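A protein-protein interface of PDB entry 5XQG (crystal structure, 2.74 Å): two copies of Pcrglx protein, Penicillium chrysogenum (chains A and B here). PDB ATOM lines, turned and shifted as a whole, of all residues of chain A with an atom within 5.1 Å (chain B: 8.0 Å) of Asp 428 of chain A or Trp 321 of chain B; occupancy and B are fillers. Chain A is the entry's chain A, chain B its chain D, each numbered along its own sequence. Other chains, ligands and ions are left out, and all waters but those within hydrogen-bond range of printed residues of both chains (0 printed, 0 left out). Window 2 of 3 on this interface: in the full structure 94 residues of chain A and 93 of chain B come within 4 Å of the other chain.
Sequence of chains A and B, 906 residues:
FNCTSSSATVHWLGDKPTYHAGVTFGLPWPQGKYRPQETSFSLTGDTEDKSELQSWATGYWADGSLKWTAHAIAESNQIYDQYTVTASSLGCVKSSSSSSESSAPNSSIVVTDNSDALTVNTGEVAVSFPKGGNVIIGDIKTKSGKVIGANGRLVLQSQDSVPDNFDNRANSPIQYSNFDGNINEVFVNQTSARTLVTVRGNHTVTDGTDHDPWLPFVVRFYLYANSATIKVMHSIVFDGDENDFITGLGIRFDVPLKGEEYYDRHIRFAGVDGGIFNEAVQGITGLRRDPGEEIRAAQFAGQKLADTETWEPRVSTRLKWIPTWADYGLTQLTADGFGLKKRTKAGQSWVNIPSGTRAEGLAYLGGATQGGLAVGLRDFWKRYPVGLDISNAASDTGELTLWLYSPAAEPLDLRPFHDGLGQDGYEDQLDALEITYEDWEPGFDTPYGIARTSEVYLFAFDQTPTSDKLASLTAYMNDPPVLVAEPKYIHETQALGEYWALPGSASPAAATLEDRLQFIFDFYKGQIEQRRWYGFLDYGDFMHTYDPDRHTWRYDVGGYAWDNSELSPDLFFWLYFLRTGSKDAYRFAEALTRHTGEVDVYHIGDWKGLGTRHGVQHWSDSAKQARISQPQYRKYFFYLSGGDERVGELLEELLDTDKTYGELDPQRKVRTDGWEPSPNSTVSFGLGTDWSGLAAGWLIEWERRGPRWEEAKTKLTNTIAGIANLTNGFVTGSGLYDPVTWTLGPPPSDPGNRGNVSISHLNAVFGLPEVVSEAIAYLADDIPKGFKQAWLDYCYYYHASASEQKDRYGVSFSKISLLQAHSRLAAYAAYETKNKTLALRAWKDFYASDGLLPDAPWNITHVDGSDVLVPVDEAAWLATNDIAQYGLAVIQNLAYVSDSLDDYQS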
ATOM      1  N   GLY A 420     -10.762 -12.435 -26.349  1.00  0.00           N
ATOM      2  CA  GLY A 420     -11.290 -11.262 -25.652  1.00  0.00           C
ATOM      3  C   GLY A 420     -10.907  -9.985 -26.363  1.00  0.00           C
ATOM      4  O   GLY A 420     -11.378  -8.913 -25.995  1.00  0.00           O
ATOM      5  N   LEU A 421     -10.027 -10.100 -27.357  1.00  0.00           N
ATOM      6  CA  LEU A 421      -9.696  -9.032 -28.281  1.00  0.00           C
ATOM      7  C   LEU A 421      -9.040  -7.846 -27.593  1.00  0.00           C
ATOM      8  O   LEU A 421      -9.107  -6.746 -28.106  1.00  0.00           O
ATOM      9  CB  LEU A 421     -10.951  -8.585 -29.046  1.00  0.00           C
ATOM     10  CG  LEU A 421     -11.998  -9.648 -29.441  1.00  0.00           C
ATOM     11  CD1 LEU A 421     -13.344  -8.993 -29.834  1.00  0.00           C
ATOM     12  CD2 LEU A 421     -11.467 -10.579 -30.527  1.00  0.00           C
ATOM     13  N   GLY A 422      -8.411  -8.072 -26.433  1.00  0.00           N
ATOM     14  CA  GLY A 422      -7.767  -6.996 -25.668  1.00  0.00           C
ATOM     15  C   GLY A 422      -8.715  -6.080 -24.904  1.00  0.00           C
ATOM     16  O   GLY A 422      -8.380  -4.938 -24.591  1.00  0.00           O
ATOM     17  N   GLN A 423      -9.900  -6.577 -24.618  1.00  0.00           N
ATOM     18  CA  GLN A 423     -10.812  -5.886 -23.770  1.00  0.00           C
ATOM     19  C   GLN A 423     -10.232  -6.010 -22.398  1.00  0.00           C
ATOM     20  O   GLN A 423      -9.885  -7.119 -21.980  1.00  0.00           O
ATOM     21  CB  GLN A 423     -12.195  -6.535 -23.772  1.00  0.00           C
ATOM     22  CG  GLN A 423     -13.103  -6.087 -24.899  1.00  0.00           C
ATOM     23  CD  GLN A 423     -14.300  -7.011 -25.057  1.00  0.00           C
ATOM     24  OE1 GLN A 423     -15.185  -7.090 -24.180  1.00  0.00           O
ATOM     25  NE2 GLN A 423     -14.339  -7.717 -26.172  1.00  0.00           N
ATOM     26  N   ASP A 424     -10.134  -4.866 -21.720  1.00  0.00           N
ATOM     27  CA  ASP A 424      -9.557  -4.763 -20.396  1.00  0.00           C
ATOM     28  C   ASP A 424     -10.513  -3.916 -19.566  1.00  0.00           C
ATOM     29  O   ASP A 424     -10.435  -2.691 -19.558  1.00  0.00           O
ATOM     30  CB  ASP A 424      -8.157  -4.136 -20.508  1.00  0.00           C
ATOM     31  CG  ASP A 424      -7.334  -4.233 -19.213  1.00  0.00           C
ATOM     32  OD1 ASP A 424      -7.772  -4.871 -18.207  1.00  0.00           O
ATOM     33  OD2 ASP A 424      -6.221  -3.649 -19.237  1.00  0.00           O
ATOM     34  N   GLY A 425     -11.466  -4.594 -18.930  1.00  0.00           N
ATOM     35  CA  GLY A 425     -12.418  -3.963 -18.015  1.00  0.00           C
ATOM     36  C   GLY A 425     -13.808  -3.667 -18.546  1.00  0.00           C
ATOM     37  O   GLY A 425     -14.075  -3.773 -19.733  1.00  0.00           O
ATOM     38  N   TYR A 426     -14.686  -3.274 -17.630  1.00  0.00           N
ATOM     39  CA  TYR A 426     -16.099  -3.018 -17.926  1.00  0.00           C
ATOM     40  C   TYR A 426     -16.340  -2.037 -19.081  1.00  0.00           C
ATOM     41  O   TYR A 426     -17.241  -2.223 -19.897  1.00  0.00           O
ATOM     42  CB  TYR A 426     -16.819  -2.516 -16.647  1.00  0.00           C
ATOM     43  CG  TYR A 426     -16.952  -3.526 -15.497  1.00  0.00           C
ATOM     44  CD1 TYR A 426     -16.616  -4.876 -15.662  1.00  0.00           C
ATOM     45  CD2 TYR A 426     -17.440  -3.118 -14.233  1.00  0.00           C
ATOM     46  CE1 TYR A 426     -16.747  -5.769 -14.627  1.00  0.00           C
ATOM     47  CE2 TYR A 426     -17.566  -4.016 -13.192  1.00  0.00           C
ATOM     48  CZ  TYR A 426     -17.217  -5.344 -13.404  1.00  0.00           C
ATOM     49  OH  TYR A 426     -17.341  -6.285 -12.410  1.00  0.00           O
ATOM     50  N   GLU A 427     -15.533  -0.994 -19.139  1.00  0.00           N
ATOM     51  CA  GLU A 427     -15.720   0.051 -20.118  1.00  0.00           C
ATOM     52  C   GLU A 427     -15.480  -0.525 -21.516  1.00  0.00           C
ATOM     53  O   GLU A 427     -16.271  -0.298 -22.418  1.00  0.00           O
ATOM     54  CB  GLU A 427     -14.779   1.222 -19.824  1.00  0.00           C
ATOM     55  CG  GLU A 427     -15.379   2.601 -20.053  1.00  0.00           C
ATOM     56  CD  GLU A 427     -14.336   3.675 -20.407  1.00  0.00           C
ATOM     57  OE1 GLU A 427     -13.109   3.397 -20.539  1.00  0.00           O
ATOM     58  OE2 GLU A 427     -14.765   4.830 -20.570  1.00  0.00           O
ATOM     59  N   ASP A 428     -14.405  -1.286 -21.690  1.00  0.00           N
ATOM     60  CA  ASP A 428     -14.123  -1.928 -22.981  1.00  0.00           C
ATOM     61  C   ASP A 428     -15.194  -2.985 -23.305  1.00  0.00           C
ATOM     62  O   ASP A 428     -15.579  -3.137 -24.461  1.00  0.00           O
ATOM     63  CB  ASP A 428     -12.736  -2.623 -23.012  1.00  0.00           C
ATOM     64  CG  ASP A 428     -11.564  -1.675 -23.177  1.00  0.00           C
ATOM     65  OD1 ASP A 428     -11.733  -0.480 -23.504  1.00  0.00           O
ATOM     66  OD2 ASP A 428     -10.431  -2.173 -22.978  1.00  0.00           O
ATOM     67  N   GLN A 429     -15.651  -3.715 -22.293  1.00  0.00           N
ATOM     68  CA  GLN A 429     -16.665  -4.745 -22.487  1.00  0.00           C
ATOM     69  C   GLN A 429     -18.005  -4.195 -22.961  1.00  0.00           C
ATOM     70  O   GLN A 429     -18.592  -4.721 -23.880  1.00  0.00           O
ATOM     71  CB  GLN A 429     -16.851  -5.534 -21.195  1.00  0.00           C
ATOM     72  CG  GLN A 429     -15.626  -6.360 -20.826  1.00  0.00           C
ATOM     73  CD  GLN A 429     -15.525  -6.712 -19.355  1.00  0.00           C
ATOM     74  OE1 GLN A 429     -16.434  -6.461 -18.543  1.00  0.00           O
ATOM     75  NE2 GLN A 429     -14.385  -7.295 -18.997  1.00  0.00           N
ATOM     76  N   LEU A 430     -18.472  -3.120 -22.357  1.00  0.00           N
ATOM     77  CA  LEU A 430     -19.734  -2.515 -22.770  1.00  0.00           C
ATOM     78  C   LEU A 430     -19.621  -1.730 -24.058  1.00  0.00           C
ATOM     79  O   LEU A 430     -20.632  -1.401 -24.669  1.00  0.00           O
ATOM     80  CB  LEU A 430     -20.265  -1.590 -21.685  1.00  0.00           C
ATOM     81  CG  LEU A 430     -20.535  -2.254 -20.332  1.00  0.00           C
ATOM     82  CD1 LEU A 430     -20.645  -1.193 -19.228  1.00  0.00           C
ATOM     83  CD2 LEU A 430     -21.763  -3.155 -20.453  1.00  0.00           C
ATOM     84  N   ASP A 431     -18.406  -1.361 -24.431  1.00  0.00           N
ATOM     85  CA  ASP A 431     -18.153  -0.764 -25.746  1.00  0.00           C
ATOM     86  C   ASP A 431     -18.277  -1.818 -26.859  1.00  0.00           C
ATOM     87  O   ASP A 431     -18.699  -1.498 -27.978  1.00  0.00           O
ATOM     88  CB  ASP A 431     -16.755  -0.101 -25.791  1.00  0.00           C
ATOM     89  CG  ASP A 431     -16.587   0.856 -26.976  1.00  0.00           C
ATOM     90  OD1 ASP A 431     -17.485   1.704 -27.231  1.00  0.00           O
ATOM     91  OD2 ASP A 431     -15.542   0.757 -27.661  1.00  0.00           O
ATOM     92  N   ALA A 432     -17.884  -3.057 -26.557  1.00  0.00           N
ATOM     93  CA  ALA A 432     -17.983  -4.150 -27.518  1.00  0.00           C
ATOM     94  C   ALA A 432     -19.441  -4.590 -27.631  1.00  0.00           C
ATOM     95  O   ALA A 432     -19.916  -4.955 -28.712  1.00  0.00           O
ATOM     96  CB  ALA A 432     -17.099  -5.307 -27.081  1.00  0.00           C
ATOM     97  N   ILE A 435     -21.431  -2.956 -30.437  1.00  0.00           N
ATOM     98  CA  ILE A 435     -21.287  -3.353 -31.854  1.00  0.00           C
ATOM     99  C   ILE A 435     -21.632  -4.807 -32.219  1.00  0.00           C
ATOM    100  O   ILE A 435     -22.253  -5.037 -33.269  1.00  0.00           O
ATOM    101  CB  ILE A 435     -19.891  -2.994 -32.395  1.00  0.00           C
ATOM    102  CG1 ILE A 435     -19.802  -3.193 -33.921  1.00  0.00           C
ATOM    103  CG2 ILE A 435     -18.806  -3.821 -31.742  1.00  0.00           C
ATOM    104  CD1 ILE A 435     -20.788  -2.335 -34.637  1.00  0.00           C
ATOM    105  N   THR A 436     -21.199  -5.782 -31.424  1.00  0.00           N
ATOM    106  CA  THR A 436     -21.611  -7.185 -31.662  1.00  0.00           C
ATOM    107  C   THR A 436     -22.796  -7.661 -30.815  1.00  0.00           C
ATOM    108  O   THR A 436     -23.209  -8.793 -30.990  1.00  0.00           O
ATOM    109  CB  THR A 436     -20.486  -8.183 -31.346  1.00  0.00           C
ATOM    110  OG1 THR A 436     -20.105  -7.992 -29.997  1.00  0.00           O
ATOM    111  CG2 THR A 436     -19.284  -7.958 -32.237  1.00  0.00           C
ATOM    112  N   GLN B 282     -13.241  -9.849 -41.671  1.00  0.00           N
ATOM    113  CA  GLN B 282     -13.932  -9.045 -40.690  1.00  0.00           C
ATOM    114  C   GLN B 282     -15.305  -8.599 -41.242  1.00  0.00           C
ATOM    115  O   GLN B 282     -15.412  -7.674 -42.071  1.00  0.00           O
ATOM    116  CB  GLN B 282     -13.093  -7.864 -40.282  1.00  0.00           C
ATOM    117  CG  GLN B 282     -13.527  -7.280 -38.950  1.00  0.00           C
ATOM    118  CD  GLN B 282     -12.657  -6.121 -38.475  1.00  0.00           C
ATOM    119  OE1 GLN B 282     -12.412  -5.954 -37.279  1.00  0.00           O
ATOM    120  NE2 GLN B 282     -12.234  -5.299 -39.404  1.00  0.00           N
ATOM    121  N   LEU B 287     -24.178  -6.541 -37.804  1.00  0.00           N
ATOM    122  CA  LEU B 287     -23.780  -5.974 -36.514  1.00  0.00           C
ATOM    123  C   LEU B 287     -24.952  -5.244 -35.873  1.00  0.00           C
ATOM    124  O   LEU B 287     -25.995  -5.021 -36.500  1.00  0.00           O
ATOM    125  CB  LEU B 287     -22.637  -4.983 -36.721  1.00  0.00           C
ATOM    126  CG  LEU B 287     -21.454  -5.471 -37.549  1.00  0.00           C
ATOM    127  CD1 LEU B 287     -20.528  -4.305 -37.870  1.00  0.00           C
ATOM    128  CD2 LEU B 287     -20.720  -6.578 -36.811  1.00  0.00           C
ATOM    129  N   ARG B 314     -20.366   5.051 -35.133  1.00  0.00           N
ATOM    130  CA  ARG B 314     -20.636   4.037 -34.107  1.00  0.00           C
ATOM    131  C   ARG B 314     -20.133   2.634 -34.525  1.00  0.00           C
ATOM    132  O   ARG B 314     -20.023   1.755 -33.660  1.00  0.00           O
ATOM    133  CB  ARG B 314     -22.121   4.022 -33.727  1.00  0.00           C
ATOM    134  CG  ARG B 314     -22.562   5.291 -32.989  1.00  0.00           C
ATOM    135  CD  ARG B 314     -24.058   5.287 -32.668  1.00  0.00           C
ATOM    136  NE  ARG B 314     -24.863   5.201 -33.901  1.00  0.00           N
ATOM    137  CZ  ARG B 314     -26.175   4.966 -33.969  1.00  0.00           C
ATOM    138  NH1 ARG B 314     -26.901   4.786 -32.871  1.00  0.00           N
ATOM    139  NH2 ARG B 314     -26.756   4.894 -35.156  1.00  0.00           N
ATOM    140  N   VAL B 315     -19.845   2.443 -35.829  1.00  0.00           N
ATOM    141  CA  VAL B 315     -19.209   1.236 -36.352  1.00  0.00           C
ATOM    142  C   VAL B 315     -17.695   1.336 -36.571  1.00  0.00           C
ATOM    143  O   VAL B 315     -16.947   0.484 -36.088  1.00  0.00           O
ATOM    144  CB  VAL B 315     -19.834   0.834 -37.692  1.00  0.00           C
ATOM    145  CG1 VAL B 315     -19.100  -0.377 -38.303  1.00  0.00           C
ATOM    146  CG2 VAL B 315     -21.330   0.550 -37.515  1.00  0.00           C
ATOM    147  N   THR B 317     -15.458   3.337 -35.513  1.00  0.00           N
ATOM    148  CA  THR B 317     -14.654   3.491 -34.278  1.00  0.00           C
ATOM    149  C   THR B 317     -14.596   2.235 -33.388  1.00  0.00           C
ATOM    150  O   THR B 317     -13.966   2.275 -32.340  1.00  0.00           O
ATOM    151  CB  THR B 317     -15.133   4.681 -33.408  1.00  0.00           C
ATOM    152  OG1 THR B 317     -16.416   4.376 -32.857  1.00  0.00           O
ATOM    153  CG2 THR B 317     -15.192   6.002 -34.227  1.00  0.00           C
ATOM    154  N   ARG B 318     -15.254   1.146 -33.786  1.00  0.00           N
ATOM    155  CA  ARG B 318     -15.365  -0.046 -32.947  1.00  0.00           C
ATOM    156  C   ARG B 318     -14.879  -1.318 -33.631  1.00  0.00           C
ATOM    157  O   ARG B 318     -15.108  -2.437 -33.135  1.00  0.00           O
ATOM    158  CB  ARG B 318     -16.817  -0.201 -32.487  1.00  0.00           C
ATOM    159  CG  ARG B 318     -17.311   0.951 -31.633  1.00  0.00           C
ATOM    160  CD  ARG B 318     -18.246   0.411 -30.589  1.00  0.00           C
ATOM    161  NE  ARG B 318     -18.789   1.394 -29.657  1.00  0.00           N
ATOM    162  CZ  ARG B 318     -19.852   2.165 -29.888  1.00  0.00           C
ATOM    163  NH1 ARG B 318     -20.506   2.155 -31.066  1.00  0.00           N
ATOM    164  NH2 ARG B 318     -20.258   2.982 -28.926  1.00  0.00           N
ATOM    165  N   LEU B 319     -14.174  -1.143 -34.748  1.00  0.00           N
ATOM    166  CA  LEU B 319     -13.670  -2.267 -35.546  1.00  0.00           C
ATOM    167  C   LEU B 319     -12.805  -3.201 -34.738  1.00  0.00           C
ATOM    168  O   LEU B 319     -12.838  -4.396 -34.960  1.00  0.00           O
ATOM    169  CB  LEU B 319     -12.911  -1.782 -36.793  1.00  0.00           C
ATOM    170  CG  LEU B 319     -13.782  -1.297 -37.974  1.00  0.00           C
ATOM    171  CD1 LEU B 319     -12.992  -0.443 -38.953  1.00  0.00           C
ATOM    172  CD2 LEU B 319     -14.384  -2.474 -38.710  1.00  0.00           C
ATOM    173  N   LYS B 320     -12.049  -2.651 -33.797  1.00  0.00           N
ATOM    174  CA  LYS B 320     -11.201  -3.441 -32.897  1.00  0.00           C
ATOM    175  C   LYS B 320     -11.948  -4.616 -32.247  1.00  0.00           C
ATOM    176  O   LYS B 320     -11.399  -5.714 -32.152  1.00  0.00           O
ATOM    177  CB  LYS B 320     -10.515  -2.555 -31.836  1.00  0.00           C
ATOM    178  CG  LYS B 320     -11.342  -1.422 -31.169  1.00  0.00           C
ATOM    179  CD  LYS B 320     -10.564  -0.810 -29.977  1.00  0.00           C
ATOM    180  CE  LYS B 320     -11.349   0.191 -29.136  1.00  0.00           C
ATOM    181  NZ  LYS B 320     -11.045   1.617 -29.432  1.00  0.00           N
ATOM    182  N   TRP B 321     -13.205  -4.385 -31.857  1.00  0.00           N
ATOM    183  CA  TRP B 321     -14.040  -5.370 -31.127  1.00  0.00           C
ATOM    184  C   TRP B 321     -14.844  -6.349 -32.008  1.00  0.00           C
ATOM    185  O   TRP B 321     -15.587  -7.209 -31.490  1.00  0.00           O
ATOM    186  CB  TRP B 321     -15.063  -4.647 -30.222  1.00  0.00           C
ATOM    187  CG  TRP B 321     -14.531  -3.596 -29.281  1.00  0.00           C
ATOM    188  CD1 TRP B 321     -15.094  -2.359 -29.044  1.00  0.00           C
ATOM    189  CD2 TRP B 321     -13.358  -3.664 -28.465  1.00  0.00           C
ATOM    190  NE1 TRP B 321     -14.343  -1.663 -28.125  1.00  0.00           N
ATOM    191  CE2 TRP B 321     -13.273  -2.436 -27.752  1.00  0.00           C
ATOM    192  CE3 TRP B 321     -12.370  -4.625 -28.265  1.00  0.00           C
ATOM    193  CZ2 TRP B 321     -12.257  -2.169 -26.825  1.00  0.00           C
ATOM    194  CZ3 TRP B 321     -11.342  -4.354 -27.349  1.00  0.00           C
ATOM    195  CH2 TRP B 321     -11.302  -3.134 -26.642  1.00  0.00           C
ATOM    196  N   ILE B 322     -14.737  -6.200 -33.318  1.00  0.00           N
ATOM    197  CA  ILE B 322     -15.343  -7.139 -34.191  1.00  0.00           C
ATOM    198  C   ILE B 322     -14.321  -8.220 -34.441  1.00  0.00           C
ATOM    199  O   ILE B 322     -13.262  -7.919 -34.939  1.00  0.00           O
ATOM    200  CB  ILE B 322     -15.776  -6.528 -35.521  1.00  0.00           C
ATOM    201  CG1 ILE B 322     -16.868  -5.484 -35.299  1.00  0.00           C
ATOM    202  CG2 ILE B 322     -16.330  -7.627 -36.419  1.00  0.00           C
ATOM    203  CD1 ILE B 322     -17.152  -4.649 -36.521  1.00  0.00           C
ATOM    204  N   PRO B 323     -14.667  -9.495 -34.162  1.00  0.00           N
ATOM    205  CA  PRO B 323     -13.703 -10.579 -34.300  1.00  0.00           C
ATOM    206  C   PRO B 323     -13.142 -10.717 -35.690  1.00  0.00           C
ATOM    207  O   PRO B 323     -13.759 -10.303 -36.653  1.00  0.00           O
ATOM    208  CB  PRO B 323     -14.539 -11.820 -33.978  1.00  0.00           C
ATOM    209  CG  PRO B 323     -15.689 -11.319 -33.169  1.00  0.00           C
ATOM    210  CD  PRO B 323     -16.011 -10.040 -33.856  1.00  0.00           C
ATOM    211  N   THR B 324     -11.982 -11.352 -35.779  1.00  0.00           N
ATOM    212  CA  THR B 324     -11.279 -11.531 -37.039  1.00  0.00           C
ATOM    213  C   THR B 324     -11.212 -13.046 -37.293  1.00  0.00           C
ATOM    214  O   THR B 324     -10.888 -13.800 -36.390  1.00  0.00           O
ATOM    215  CB  THR B 324      -9.940 -10.743 -36.953  1.00  0.00           C
ATOM    216  OG1 THR B 324      -9.662 -10.131 -38.219  1.00  0.00           O
ATOM    217  CG2 THR B 324      -8.719 -11.596 -36.411  1.00  0.00           C
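No position is printed for both chains.
O of Gly 420 of chain A lies within hydrogen-bond range of NE2 of Gln 423 of chain A, at 3.2 Å. The guanidinium group (NH1) of Arg 318 of chain B sits at hydrogen-bond distance from the backbone carbonyl oxygen (O) of Arg 314 of chain B, at 2.7 Å. The backbone carbonyl oxygen of Ala 432 of chain A sits at hydrogen-bond distance from the side-chain hydroxyl of Thr 436 of chain A, at 3.3 Å. N of Asp 424 of chain A sits at hydrogen-bond distance from OD2 of Asp 428 of chain A, 3.0 Å away. The backbone carbonyl oxygen of Ile 322 of chain B sits close to the side-chain amide oxygen of Gln 282 of chain B (3.2 Å).
Gly 420 of chain A touches none of the printed residues of chain B. Printed residues of chain B within 4 Å of Leu 421 of chain A: Trp 321. Tyr 426 of chain A touches none of the printed residues of chain B. Of chain B, only Trp 321 (3.7 Å) comes within 4 Å of Asp 428 of chain A. Of the printed residues of chain B, Ile 435 of chain A touches Leu 287 and Ile 322. Printed residues of chain A within 4 Å of Trp 321 of chain B: Leu 421 (3.3 Å), Gly 422 (3.98 Å), Gln 423 (3.5 Å), Asp 428 (3.7 Å), Asp 431 (2.7 Å), Ala 432 (3.7 Å) and Thr 436 (3.8 Å).
OD2 of Asp 431 of chain A lies within hydrogen-bond range of NE1 of Trp 321 of chain B (2.7 Å). The side-chain carboxylate (OD1) of Asp 431 of chain A lies within salt-bridge range of the guanidinium group (NE) of Arg 318 of chain B (2.8 Å).
Of the 12 printed residues of chain B, 4 touch a printed residue of chain A. Printed residues of chain B that touch a printed residue of chain A: Leu 287, Arg 318, Trp 321 and Ile 322. Hydrophobic or aromatic side chains of chain B within 4 Å of the printed part of chain A: Leu 287, Trp 321 and Ile 322. Of the 15 printed residues of chain A, 8 touch a printed residue of chain B. Printed residues of chain A that touch a printed residue of chain B: Leu 421, Gly 422, Gln 423, Asp 428, Asp 431, Ala 432, Ile 435 and Thr 436. Among the printed residues, Asp or Glu carboxylates within 4 Å of a Lys or Arg side-chain nitrogen of the other chain: Asp 431 of chain A with Arg 318 of chain B.
Among the printed residues, merely in contact across the chains: Leu 421 of chain A with Trp 321 of chain B, Gly 422 of chain A with Trp 321 of chain B, Gln 423 of chain A with Trp 321 of chain B, Asp 428 of chain A with Trp 321 of chain B, Ala 432 of chain A with Trp 321 of chain B, Ile 435 of chain A with Leu 287 of chain B, Ile 435 of chain A with Ile 322 of chain B and Thr 436 of chain A with Trp 321 of chain B.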
